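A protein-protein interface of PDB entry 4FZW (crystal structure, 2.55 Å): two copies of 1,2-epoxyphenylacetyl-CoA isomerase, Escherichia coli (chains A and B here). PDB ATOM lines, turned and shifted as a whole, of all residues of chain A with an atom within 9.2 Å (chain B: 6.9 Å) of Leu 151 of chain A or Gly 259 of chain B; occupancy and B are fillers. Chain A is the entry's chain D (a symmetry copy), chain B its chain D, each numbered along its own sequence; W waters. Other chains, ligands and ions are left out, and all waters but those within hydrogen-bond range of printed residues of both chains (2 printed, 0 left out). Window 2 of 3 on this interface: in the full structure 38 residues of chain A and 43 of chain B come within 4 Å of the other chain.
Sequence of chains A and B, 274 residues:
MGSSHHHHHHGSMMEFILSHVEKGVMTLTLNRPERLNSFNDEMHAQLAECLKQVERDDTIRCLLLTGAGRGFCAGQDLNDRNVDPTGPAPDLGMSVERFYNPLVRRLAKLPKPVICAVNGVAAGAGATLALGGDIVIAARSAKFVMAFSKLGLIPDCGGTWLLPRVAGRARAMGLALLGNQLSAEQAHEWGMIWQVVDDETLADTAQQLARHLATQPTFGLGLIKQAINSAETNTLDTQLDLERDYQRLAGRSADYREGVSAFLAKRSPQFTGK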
ATOM      1  N   ALA A  74      27.337  18.918   0.035  1.00  0.00           N
ATOM      2  CA  ALA A  74      26.792  18.091  -1.045  1.00  0.00           C
ATOM      3  C   ALA A  74      25.385  17.556  -0.742  1.00  0.00           C
ATOM      4  O   ALA A  74      24.847  16.758  -1.519  1.00  0.00           O
ATOM      5  CB  ALA A  74      27.728  16.937  -1.365  1.00  0.00           C
ATOM      6  N   GLN A  76      22.372  15.505   0.968  1.00  0.00           N
ATOM      7  CA  GLN A  76      22.123  14.236   1.638  1.00  0.00           C
ATOM      8  C   GLN A  76      23.009  13.129   1.091  1.00  0.00           C
ATOM      9  O   GLN A  76      23.012  12.865  -0.110  1.00  0.00           O
ATOM     10  CB  GLN A  76      20.648  13.834   1.534  1.00  0.00           C
ATOM     11  N   ASP A  77      23.764  12.495   1.984  1.00  0.00           N
ATOM     12  CA  ASP A  77      24.574  11.337   1.630  1.00  0.00           C
ATOM     13  C   ASP A  77      23.661  10.197   1.194  1.00  0.00           C
ATOM     14  O   ASP A  77      22.864   9.685   1.992  1.00  0.00           O
ATOM     15  CB  ASP A  77      25.442  10.914   2.820  1.00  0.00           C
ATOM     16  CG  ASP A  77      26.305   9.705   2.512  1.00  0.00           C
ATOM     17  OD1 ASP A  77      27.288   9.859   1.756  1.00  0.00           O
ATOM     18  OD2 ASP A  77      26.006   8.604   3.029  1.00  0.00           O
ATOM     19  N   LEU A  78      23.775   9.806  -0.076  1.00  0.00           N
ATOM     20  CA  LEU A  78      22.837   8.850  -0.668  1.00  0.00           C
ATOM     21  C   LEU A  78      23.317   7.396  -0.683  1.00  0.00           C
ATOM     22  O   LEU A  78      23.307   6.740  -1.725  1.00  0.00           O
ATOM     23  CB  LEU A  78      22.376   9.310  -2.068  1.00  0.00           C
ATOM     24  CG  LEU A  78      23.346   9.534  -3.235  1.00  0.00           C
ATOM     25  CD1 LEU A  78      23.708   8.235  -3.940  1.00  0.00           C
ATOM     26  CD2 LEU A  78      22.731  10.503  -4.237  1.00  0.00           C
ATOM     27  N   LEU A  92      10.999   8.584   1.269  1.00  0.00           N
ATOM     28  CA  LEU A  92      11.759   9.844   1.297  1.00  0.00           C
ATOM     29  C   LEU A  92      11.022  10.937   2.075  1.00  0.00           C
ATOM     30  O   LEU A  92      11.633  11.901   2.530  1.00  0.00           O
ATOM     31  CB  LEU A  92      12.110  10.307  -0.123  1.00  0.00           C
ATOM     32  CG  LEU A  92      12.938   9.326  -0.952  1.00  0.00           C
ATOM     33  CD1 LEU A  92      13.183   9.872  -2.352  1.00  0.00           C
ATOM     34  CD2 LEU A  92      14.257   8.980  -0.264  1.00  0.00           C
ATOM     35  N   GLY A 124      22.218  19.416  -3.962  1.00  0.00           N
ATOM     36  CA  GLY A 124      20.998  18.903  -3.368  1.00  0.00           C
ATOM     37  C   GLY A 124      20.451  19.742  -2.223  1.00  0.00           C
ATOM     38  O   GLY A 124      20.171  20.935  -2.375  1.00  0.00           O
ATOM     39  N   ALA A 125      20.287  19.102  -1.069  1.00  0.00           N
ATOM     40  CA  ALA A 125      19.817  19.782   0.135  1.00  0.00           C
ATOM     41  C   ALA A 125      20.770  20.912   0.533  1.00  0.00           C
ATOM     42  O   ALA A 125      20.355  21.899   1.142  1.00  0.00           O
ATOM     43  CB  ALA A 125      19.658  18.780   1.278  1.00  0.00           C
ATOM     44  N   MET A 146      21.603  21.908  -8.111  1.00  0.00           N
ATOM     45  CA  MET A 146      20.322  21.316  -7.763  1.00  0.00           C
ATOM     46  C   MET A 146      19.904  20.314  -8.829  1.00  0.00           C
ATOM     47  O   MET A 146      19.091  20.625  -9.707  1.00  0.00           O
ATOM     48  CB  MET A 146      19.248  22.390  -7.593  1.00  0.00           C
ATOM     49  CG  MET A 146      19.493  23.301  -6.410  1.00  0.00           C
ATOM     50  SD  MET A 146      18.514  24.820  -6.492  1.00  0.00           S
ATOM     51  CE  MET A 146      19.209  25.606  -7.959  1.00  0.00           C
ATOM     52  N   ALA A 147      20.462  19.112  -8.747  1.00  0.00           N
ATOM     53  CA  ALA A 147      20.186  18.074  -9.734  1.00  0.00           C
ATOM     54  C   ALA A 147      19.109  17.086  -9.310  1.00  0.00           C
ATOM     55  O   ALA A 147      19.103  15.954  -9.782  1.00  0.00           O
ATOM     56  CB  ALA A 147      21.443  17.324 -10.071  1.00  0.00           C
ATOM     57  N   PHE A 148      18.199  17.504  -8.432  1.00  0.00           N
ATOM     58  CA  PHE A 148      17.131  16.617  -7.992  1.00  0.00           C
ATOM     59  C   PHE A 148      16.487  15.900  -9.176  1.00  0.00           C
ATOM     60  O   PHE A 148      16.438  14.676  -9.197  1.00  0.00           O
ATOM     61  CB  PHE A 148      16.070  17.364  -7.186  1.00  0.00           C
ATOM     62  CG  PHE A 148      16.616  18.087  -6.005  1.00  0.00           C
ATOM     63  CD1 PHE A 148      17.182  19.344  -6.158  1.00  0.00           C
ATOM     64  CD2 PHE A 148      16.563  17.521  -4.733  1.00  0.00           C
ATOM     65  CE1 PHE A 148      17.689  20.024  -5.069  1.00  0.00           C
ATOM     66  CE2 PHE A 148      17.066  18.198  -3.635  1.00  0.00           C
ATOM     67  CZ  PHE A 148      17.626  19.450  -3.803  1.00  0.00           C
ATOM     68  N   SER A 149      16.009  16.654 -10.163  1.00  0.00           N
ATOM     69  CA  SER A 149      15.310  16.053 -11.302  1.00  0.00           C
ATOM     70  C   SER A 149      16.071  14.882 -11.960  1.00  0.00           C
ATOM     71  O   SER A 149      15.448  13.922 -12.425  1.00  0.00           O
ATOM     72  CB  SER A 149      14.912  17.116 -12.339  1.00  0.00           C
ATOM     73  OG  SER A 149      16.038  17.849 -12.800  1.00  0.00           O
ATOM     74  N   LYS A 150      17.403  14.951 -11.992  1.00  0.00           N
ATOM     75  CA  LYS A 150      18.214  13.872 -12.573  1.00  0.00           C
ATOM     76  C   LYS A 150      17.963  12.538 -11.852  1.00  0.00           C
ATOM     77  O   LYS A 150      18.082  11.456 -12.439  1.00  0.00           O
ATOM     78  CB  LYS A 150      19.715  14.206 -12.525  1.00  0.00           C
ATOM     79  CG  LYS A 150      20.129  15.494 -13.236  1.00  0.00           C
ATOM     80  CD  LYS A 150      19.809  15.456 -14.713  1.00  0.00           C
ATOM     81  CE  LYS A 150      20.145  16.783 -15.370  1.00  0.00           C
ATOM     82  NZ  LYS A 150      21.607  17.078 -15.389  1.00  0.00           N
ATOM     83  N   LEU A 151      17.621  12.631 -10.575  1.00  0.00           N
ATOM     84  CA  LEU A 151      17.297  11.451  -9.784  1.00  0.00           C
ATOM     85  C   LEU A 151      15.805  11.139  -9.758  1.00  0.00           C
ATOM     86  O   LEU A 151      15.372  10.282  -9.009  1.00  0.00           O
ATOM     87  CB  LEU A 151      17.788  11.630  -8.353  1.00  0.00           C
ATOM     88  CG  LEU A 151      19.299  11.737  -8.258  1.00  0.00           C
ATOM     89  CD1 LEU A 151      19.715  12.002  -6.835  1.00  0.00           C
ATOM     90  CD2 LEU A 151      19.919  10.464  -8.782  1.00  0.00           C
ATOM     91  N   GLY A 152      15.034  11.833 -10.585  1.00  0.00           N
ATOM     92  CA  GLY A 152      13.587  11.705 -10.583  1.00  0.00           C
ATOM     93  C   GLY A 152      12.968  12.229  -9.297  1.00  0.00           C
ATOM     94  O   GLY A 152      11.910  11.757  -8.891  1.00  0.00           O
ATOM     95  N   LEU A 153      13.629  13.200  -8.664  1.00  0.00           N
ATOM     96  CA  LEU A 153      13.201  13.750  -7.375  1.00  0.00           C
ATOM     97  C   LEU A 153      12.801  15.215  -7.504  1.00  0.00           C
ATOM     98  O   LEU A 153      12.890  15.787  -8.580  1.00  0.00           O
ATOM     99  CB  LEU A 153      14.324  13.636  -6.338  1.00  0.00           C
ATOM    100  CG  LEU A 153      14.740  12.227  -5.920  1.00  0.00           C
ATOM    101  CD1 LEU A 153      15.571  12.299  -4.661  1.00  0.00           C
ATOM    102  CD2 LEU A 153      13.529  11.331  -5.720  1.00  0.00           C
ATOM    103  N   ILE A 154      12.377  15.813  -6.392  1.00  0.00           N
ATOM    104  CA  ILE A 154      12.050  17.236  -6.328  1.00  0.00           C
ATOM    105  C   ILE A 154      13.003  17.949  -5.383  1.00  0.00           C
ATOM    106  O   ILE A 154      13.506  17.342  -4.430  1.00  0.00           O
ATOM    107  CB  ILE A 154      10.648  17.497  -5.770  1.00  0.00           C
ATOM    108  CG1 ILE A 154      10.604  17.095  -4.294  1.00  0.00           C
ATOM    109  CG2 ILE A 154       9.603  16.778  -6.597  1.00  0.00           C
ATOM    110  CD1 ILE A 154       9.344  17.410  -3.613  1.00  0.00           C
ATOM    111  N   ALA A 176      15.029  24.099 -11.852  1.00  0.00           N
ATOM    112  CA  ALA A 176      14.545  22.921 -11.156  1.00  0.00           C
ATOM    113  C   ALA A 176      14.250  21.771 -12.117  1.00  0.00           C
ATOM    114  O   ALA A 176      14.442  20.610 -11.765  1.00  0.00           O
ATOM    115  CB  ALA A 176      13.317  23.274 -10.342  1.00  0.00           C
ATOM    116  N   LEU A 177      13.783  22.112 -13.317  1.00  0.00           N
ATOM    117  CA  LEU A 177      13.463  21.120 -14.336  1.00  0.00           C
ATOM    118  C   LEU A 177      14.709  20.536 -15.023  1.00  0.00           C
ATOM    119  O   LEU A 177      14.854  19.324 -15.134  1.00  0.00           O
ATOM    120  CB  LEU A 177      12.500  21.697 -15.378  1.00  0.00           C
ATOM    121  CG  LEU A 177      11.066  22.064 -14.932  1.00  0.00           C
ATOM    122  CD1 LEU A 177      10.275  22.646 -16.077  1.00  0.00           C
ATOM    123  CD2 LEU A 177      10.308  20.888 -14.371  1.00  0.00           C
ATOM    124  N   LEU A 178      15.623  21.388 -15.483  1.00  0.00           N
ATOM    125  CA  LEU A 178      16.805  20.894 -16.191  1.00  0.00           C
ATOM    126  C   LEU A 178      17.908  20.455 -15.229  1.00  0.00           C
ATOM    127  O   LEU A 178      18.708  19.545 -15.508  1.00  0.00           O
ATOM    128  CB  LEU A 178      17.315  21.928 -17.163  1.00  0.00           C
ATOM    129  CG  LEU A 178      16.450  22.158 -18.401  1.00  0.00           C
ATOM    130  CD1 LEU A 178      15.625  23.406 -18.211  1.00  0.00           C
ATOM    131  CD2 LEU A 178      17.347  22.327 -19.627  1.00  0.00           C
ATOM    132  N   GLY A 179      17.954  21.112 -14.083  1.00  0.00           N
ATOM    133  CA  GLY A 179      18.718  20.592 -12.968  1.00  0.00           C
ATOM    134  C   GLY A 179      20.225  20.643 -13.059  1.00  0.00           C
ATOM    135  O   GLY A 179      20.869  19.704 -12.588  1.00  0.00           O
ATOM    136  N   GLN B 216      13.710  12.122 -19.630  1.00  0.00           N
ATOM    137  CA  GLN B 216      13.985  12.390 -18.230  1.00  0.00           C
ATOM    138  C   GLN B 216      12.820  11.901 -17.347  1.00  0.00           C
ATOM    139  O   GLN B 216      11.734  11.605 -17.852  1.00  0.00           O
ATOM    140  CB  GLN B 216      14.288  13.877 -18.017  1.00  0.00           C
ATOM    141  CG  GLN B 216      15.599  14.360 -18.640  1.00  0.00           C
ATOM    142  CD  GLN B 216      16.803  13.542 -18.196  1.00  0.00           C
ATOM    143  OE1 GLN B 216      17.339  12.733 -18.965  1.00  0.00           O
ATOM    144  NE2 GLN B 216      17.239  13.752 -16.953  1.00  0.00           N
ATOM    145  N   PRO B 217      13.051  11.783 -16.028  1.00  0.00           N
ATOM    146  CA  PRO B 217      11.979  11.229 -15.179  1.00  0.00           C
ATOM    147  C   PRO B 217      10.730  12.109 -15.236  1.00  0.00           C
ATOM    148  O   PRO B 217      10.614  13.020 -14.429  1.00  0.00           O
ATOM    149  CB  PRO B 217      12.590  11.263 -13.771  1.00  0.00           C
ATOM    150  CG  PRO B 217      14.100  11.367 -14.000  1.00  0.00           C
ATOM    151  CD  PRO B 217      14.239  12.189 -15.250  1.00  0.00           C
ATOM    152  N   ALA B 250       7.771  10.642  -5.218  1.00  0.00           N
ATOM    153  CA  ALA B 250       8.854  10.521  -6.203  1.00  0.00           C
ATOM    154  C   ALA B 250       9.747   9.329  -5.888  1.00  0.00           C
ATOM    155  O   ALA B 250      10.094   8.562  -6.775  1.00  0.00           O
ATOM    156  CB  ALA B 250       9.669  11.789  -6.276  1.00  0.00           C
ATOM    157  N   GLY B 251      10.103   9.170  -4.619  1.00  0.00           N
ATOM    158  CA  GLY B 251      10.990   8.091  -4.193  1.00  0.00           C
ATOM    159  C   GLY B 251      10.437   6.667  -4.293  1.00  0.00           C
ATOM    160  O   GLY B 251      11.085   5.726  -3.845  1.00  0.00           O
ATOM    161  N   SER B 253       8.892   5.941  -7.344  1.00  0.00           N
ATOM    162  CA  SER B 253       8.864   5.770  -8.798  1.00  0.00           C
ATOM    163  C   SER B 253       9.932   4.784  -9.250  1.00  0.00           C
ATOM    164  O   SER B 253      10.930   4.576  -8.553  1.00  0.00           O
ATOM    165  CB  SER B 253       9.027   7.115  -9.527  1.00  0.00           C
ATOM    166  OG  SER B 253      10.262   7.736  -9.213  1.00  0.00           O
ATOM    167  N   ALA B 254       9.706   4.154 -10.402  1.00  0.00           N
ATOM    168  CA  ALA B 254      10.744   3.322 -11.035  1.00  0.00           C
ATOM    169  C   ALA B 254      11.992   4.168 -11.295  1.00  0.00           C
ATOM    170  O   ALA B 254      13.102   3.740 -10.997  1.00  0.00           O
ATOM    171  CB  ALA B 254      10.243   2.692 -12.347  1.00  0.00           C
ATOM    172  N   ASP B 255      11.799   5.371 -11.835  1.00  0.00           N
ATOM    173  CA  ASP B 255      12.916   6.263 -12.192  1.00  0.00           C
ATOM    174  C   ASP B 255      13.810   6.680 -11.018  1.00  0.00           C
ATOM    175  O   ASP B 255      14.983   6.977 -11.211  1.00  0.00           O
ATOM    176  CB  ASP B 255      12.415   7.505 -12.934  1.00  0.00           C
ATOM    177  CG  ASP B 255      11.873   7.185 -14.308  1.00  0.00           C
ATOM    178  OD1 ASP B 255      12.151   6.074 -14.814  1.00  0.00           O
ATOM    179  OD2 ASP B 255      11.184   8.052 -14.894  1.00  0.00           O
ATOM    180  N   TYR B 256      13.271   6.729  -9.806  1.00  0.00           N
ATOM    181  CA  TYR B 256      14.137   7.008  -8.673  1.00  0.00           C
ATOM    182  C   TYR B 256      15.129   5.862  -8.537  1.00  0.00           C
ATOM    183  O   TYR B 256      16.346   6.070  -8.494  1.00  0.00           O
ATOM    184  CB  TYR B 256      13.356   7.177  -7.368  1.00  0.00           C
ATOM    185  CG  TYR B 256      14.278   7.291  -6.175  1.00  0.00           C
ATOM    186  CD1 TYR B 256      15.186   8.342  -6.087  1.00  0.00           C
ATOM    187  CD2 TYR B 256      14.287   6.331  -5.163  1.00  0.00           C
ATOM    188  CE1 TYR B 256      16.073   8.454  -5.007  1.00  0.00           C
ATOM    189  CE2 TYR B 256      15.161   6.432  -4.079  1.00  0.00           C
ATOM    190  CZ  TYR B 256      16.056   7.501  -4.007  1.00  0.00           C
ATOM    191  OH  TYR B 256      16.936   7.627  -2.944  1.00  0.00           O
ATOM    192  N   ARG B 257      14.596   4.642  -8.483  1.00  0.00           N
ATOM    193  CA  ARG B 257      15.420   3.439  -8.334  1.00  0.00           C
ATOM    194  C   ARG B 257      16.459   3.344  -9.451  1.00  0.00           C
ATOM    195  O   ARG B 257      17.637   3.085  -9.194  1.00  0.00           O
ATOM    196  CB  ARG B 257      14.543   2.170  -8.271  1.00  0.00           C
ATOM    197  N   GLU B 258      16.010   3.581 -10.680  1.00  0.00           N
ATOM    198  CA  GLU B 258      16.871   3.544 -11.853  1.00  0.00           C
ATOM    199  C   GLU B 258      17.983   4.573 -11.730  1.00  0.00           C
ATOM    200  O   GLU B 258      19.134   4.275 -12.020  1.00  0.00           O
ATOM    201  CB  GLU B 258      16.041   3.761 -13.131  1.00  0.00           C
ATOM    202  CG  GLU B 258      16.826   3.950 -14.427  1.00  0.00           C
ATOM    203  CD  GLU B 258      17.892   2.881 -14.685  1.00  0.00           C
ATOM    204  OE1 GLU B 258      17.946   1.874 -13.942  1.00  0.00           O
ATOM    205  OE2 GLU B 258      18.694   3.063 -15.637  1.00  0.00           O
ATOM    206  N   GLY B 259      17.631   5.772 -11.268  1.00  0.00           N
ATOM    207  CA  GLY B 259      18.553   6.898 -11.186  1.00  0.00           C
ATOM    208  C   GLY B 259      19.658   6.766 -10.155  1.00  0.00           C
ATOM    209  O   GLY B 259      20.790   7.185 -10.382  1.00  0.00           O
ATOM    210  N   VAL B 260      19.322   6.183  -9.014  1.00  0.00           N
ATOM    211  CA  VAL B 260      20.310   5.893  -7.982  1.00  0.00           C
ATOM    212  C   VAL B 260      21.174   4.668  -8.331  1.00  0.00           C
ATOM    213  O   VAL B 260      22.269   4.544  -7.806  1.00  0.00           O
ATOM    214  CB  VAL B 260      19.649   5.690  -6.584  1.00  0.00           C
ATOM    215  CG1 VAL B 260      20.703   5.312  -5.475  1.00  0.00           C
ATOM    216  CG2 VAL B 260      18.850   6.942  -6.159  1.00  0.00           C
ATOM    217  N   SER B 261      20.710   3.767  -9.203  1.00  0.00           N
ATOM    218  CA  SER B 261      21.566   2.636  -9.592  1.00  0.00           C
ATOM    219  C   SER B 261      22.475   2.975 -10.774  1.00  0.00           C
ATOM    220  O   SER B 261      23.656   2.624 -10.767  1.00  0.00           O
ATOM    221  CB  SER B 261      20.791   1.340  -9.853  1.00  0.00           C
ATOM    222  OG  SER B 261      19.976   1.424 -11.022  1.00  0.00           O
ATOM    223  N   ALA B 262      21.928   3.660 -11.778  1.00  0.00           N
ATOM    224  CA  ALA B 262      22.734   4.207 -12.873  1.00  0.00           C
ATOM    225  C   ALA B 262      23.910   5.050 -12.355  1.00  0.00           C
ATOM    226  O   ALA B 262      25.054   4.865 -12.773  1.00  0.00           O
ATOM    227  CB  ALA B 262      21.861   5.020 -13.840  1.00  0.00           C
ATOM    228  N   PHE B 263      23.619   5.978 -11.452  1.00  0.00           N
ATOM    229  CA  PHE B 263      24.655   6.794 -10.838  1.00  0.00           C
ATOM    230  C   PHE B 263      25.696   5.988 -10.059  1.00  0.00           C
ATOM    231  O   PHE B 263      26.901   6.165 -10.257  1.00  0.00           O
ATOM    232  CB  PHE B 263      24.028   7.813  -9.902  1.00  0.00           C
ATOM    233  CG  PHE B 263      25.045   8.654  -9.180  1.00  0.00           C
ATOM    234  CD1 PHE B 263      25.795   9.592  -9.873  1.00  0.00           C
ATOM    235  CD2 PHE B 263      25.291   8.482  -7.814  1.00  0.00           C
ATOM    236  CE1 PHE B 263      26.780  10.363  -9.214  1.00  0.00           C
ATOM    237  CE2 PHE B 263      26.286   9.272  -7.151  1.00  0.00           C
ATOM    238  CZ  PHE B 263      27.009  10.202  -7.855  1.00  0.00           C
ATOM    239  N   LEU B 264      25.229   5.130  -9.153  1.00  0.00           N
ATOM    240  CA  LEU B 264      26.127   4.235  -8.427  1.00  0.00           C
ATOM    241  C   LEU B 264      26.981   3.405  -9.399  1.00  0.00           C
ATOM    242  O   LEU B 264      28.137   3.121  -9.107  1.00  0.00           O
ATOM    243  CB  LEU B 264      25.373   3.313  -7.455  1.00  0.00           C
ATOM    244  CG  LEU B 264      24.845   3.819  -6.083  1.00  0.00           C
ATOM    245  CD1 LEU B 264      24.038   2.812  -5.401  1.00  0.00           C
ATOM    246  CD2 LEU B 264      26.066   4.221  -5.233  1.00  0.00           C
ATOM    247  N   ARG B 267      26.815   4.431 -15.069  1.00  0.00           N
ATOM    248  CA  ARG B 267      26.197   4.241 -16.374  1.00  0.00           C
ATOM    249  C   ARG B 267      25.062   5.226 -16.598  1.00  0.00           C
ATOM    250  O   ARG B 267      24.555   5.835 -15.672  1.00  0.00           O
ATOM    251  CB  ARG B 267      25.625   2.832 -16.541  1.00  0.00           C
ATOM    252  CG  ARG B 267      24.299   2.602 -15.656  1.00  0.00           C
ATOM    253  CD  ARG B 267      23.996   1.125 -15.522  1.00  0.00           C
ATOM    254  NE  ARG B 267      23.030   0.945 -14.423  1.00  0.00           N
ATOM    255  CZ  ARG B 267      21.724   1.225 -14.515  1.00  0.00           C
ATOM    256  NH1 ARG B 267      21.233   1.672 -15.674  1.00  0.00           N
ATOM    257  NH2 ARG B 267      20.921   1.086 -13.454  1.00  0.00           N
ATOM    258  N   PRO B 269      21.367   6.467 -17.354  1.00  0.00           N
ATOM    259  CA  PRO B 269      20.098   5.976 -16.819  1.00  0.00           C
ATOM    260  C   PRO B 269      19.066   5.857 -17.932  1.00  0.00           C
ATOM    261  O   PRO B 269      19.073   6.657 -18.858  1.00  0.00           O
ATOM    262  CB  PRO B 269      19.694   7.085 -15.833  1.00  0.00           C
ATOM    263  CG  PRO B 269      20.195   8.313 -16.440  1.00  0.00           C
ATOM    264  CD  PRO B 269      21.452   7.940 -17.268  1.00  0.00           C
ATOM    265  N   GLN B 270      18.207   4.847 -17.858  1.00  0.00           N
ATOM    266  CA  GLN B 270      17.092   4.719 -18.797  1.00  0.00           C
ATOM    267  C   GLN B 270      15.750   4.923 -18.107  1.00  0.00           C
ATOM    268  O   GLN B 270      15.140   3.970 -17.634  1.00  0.00           O
ATOM    269  CB  GLN B 270      17.092   3.347 -19.473  1.00  0.00           C
ATOM    270  CG  GLN B 270      18.225   3.174 -20.446  1.00  0.00           C
ATOM    271  CD  GLN B 270      18.663   1.716 -20.546  1.00  0.00           C
ATOM    272  OE1 GLN B 270      18.679   0.978 -19.560  1.00  0.00           O
ATOM    273  NE2 GLN B 270      19.034   1.306 -21.735  1.00  0.00           N
ATOM    274  N   PHE B 271      15.296   6.170 -18.065  1.00  0.00           N
ATOM    275  CA  PHE B 271      14.022   6.508 -17.445  1.00  0.00           C
ATOM    276  C   PHE B 271      12.835   6.108 -18.324  1.00  0.00           C
ATOM    277  O   PHE B 271      12.921   6.162 -19.554  1.00  0.00           O
ATOM    278  CB  PHE B 271      13.978   8.003 -17.109  1.00  0.00           C
ATOM    279  CG  PHE B 271      15.098   8.455 -16.200  1.00  0.00           C
ATOM    280  CD1 PHE B 271      15.202   7.972 -14.909  1.00  0.00           C
ATOM    281  CD2 PHE B 271      16.048   9.363 -16.645  1.00  0.00           C
ATOM    282  CE1 PHE B 271      16.230   8.380 -14.072  1.00  0.00           C
ATOM    283  CE2 PHE B 271      17.091   9.786 -15.806  1.00  0.00           C
ATOM    284  CZ  PHE B 271      17.183   9.291 -14.526  1.00  0.00           C
HETATM  285  O   HOH W   1      10.365  10.190 -10.440  1.00  0.00           O
HETATM  286  O   HOH W   2      15.854  15.941 -15.441  1.00  0.00           O
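The backbone NH of Leu 153 of chain A sits at hydrogen-bond distance from the backbone carbonyl oxygen of Phe 148 of chain A (3.2 Å).
The side-chain hydroxyl of Ser 253 of chain B sits at hydrogen-bond distance from the backbone carbonyl oxygen of Ala 250 of chain B, at 2.6 Å.
The side-chain hydroxyl of Ser 149 of chain A is in hydrogen-bond range of the backbone carbonyl oxygen of Ala 176 of chain A, 3.4 Å away.
OG of Ser 149 of chain A sits at hydrogen-bond distance from O of Leu 177 of chain A, 3.0 Å away.
N of Tyr 256 of chain B sits at hydrogen-bond distance from OG of Ser 253 of chain B, at 3.2 Å.
Printed residues of chain A that touch a printed residue of chain B: Leu 92, Ser 149, Lys 150, Leu 151, Gly 152 and Leu 153.
Among the printed residues, 11 pairs touch across the chains.
Among the printed residues, no Asp or Glu carboxylate lies within 4 Å of a Lys or Arg side-chain nitrogen of the other chain.
Of the printed residues of chain B, Leu 151 of chain A touches Asp 255, Tyr 256 and Gly 259.
Printed residues of chain A within 4 Å of Gly 259 of chain B: Leu 151 (3.8 Å).
No residue of chain A comes within 4 Å of Val 260 of chain B.
Of the printed residues of chain A, Pro 217 of chain B touches Ser 149 and Gly 152.
Printed residues of chain B within 4 Å of Ser 149 of chain A: Pro 217.
Printed residues of chain A within 4 Å of Phe 271 of chain B: Lys 150.
Printed residues of chain B within 4 Å of Leu 92 of chain A: Gly 251 (3.4 Å).
Of the printed residues of chain B, Lys 150 of chain A touches Gln 216 and Phe 271.
The nearest residue of chain A that does not touch Gly 259 of chain B is Lys 150 of chain A (4.8 Å).
The nearest printed residue of chain A that does not touch Phe 271 of chain B is Gly 152 of chain A (5.1 Å).
Leu 92 of chain A touches Gly 251 of chain B.
Ser 149 of chain A touches Pro 217 of chain B (O to CG, 3.3 Å).
Lys 150 of chain A touches Gln 216 of chain B.
O of Lys 150 of chain A touches CZ of Phe 271 of chain B, 3.1 Å away.
O of Asp 255 of chain B touches O of Leu 151 of chain A, 3.99 Å away.
CD1 of Tyr 256 of chain B touches O of Leu 151 of chain A, at 3.5 Å.
Leu 151 of chain A touches Gly 259 of chain B (CD2 to O, 3.8 Å).
Gly 152 of chain A touches Ala 250 of chain B.
Leu 153 of chain A touches Ala 250 of chain B (CD2 to CB, 3.9 Å).
Leu 153 of chain A touches Tyr 256 of chain B (CD2 to CD1, 3.4 Å).
No position is printed for both chains.
Water W1 bridges the backbone carbonyl oxygen (O) of Gly 152 of chain A (2.7 Å) and the side-chain hydroxyl (OG) of Ser 253 of chain B (2.7 Å).
Water W2 lies within hydrogen-bond range of the side-chain amide nitrogen of Gln 216 of chain B (3.0 Å) and the side-chain hydroxyl of Ser 149 of chain A (3.3 Å).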
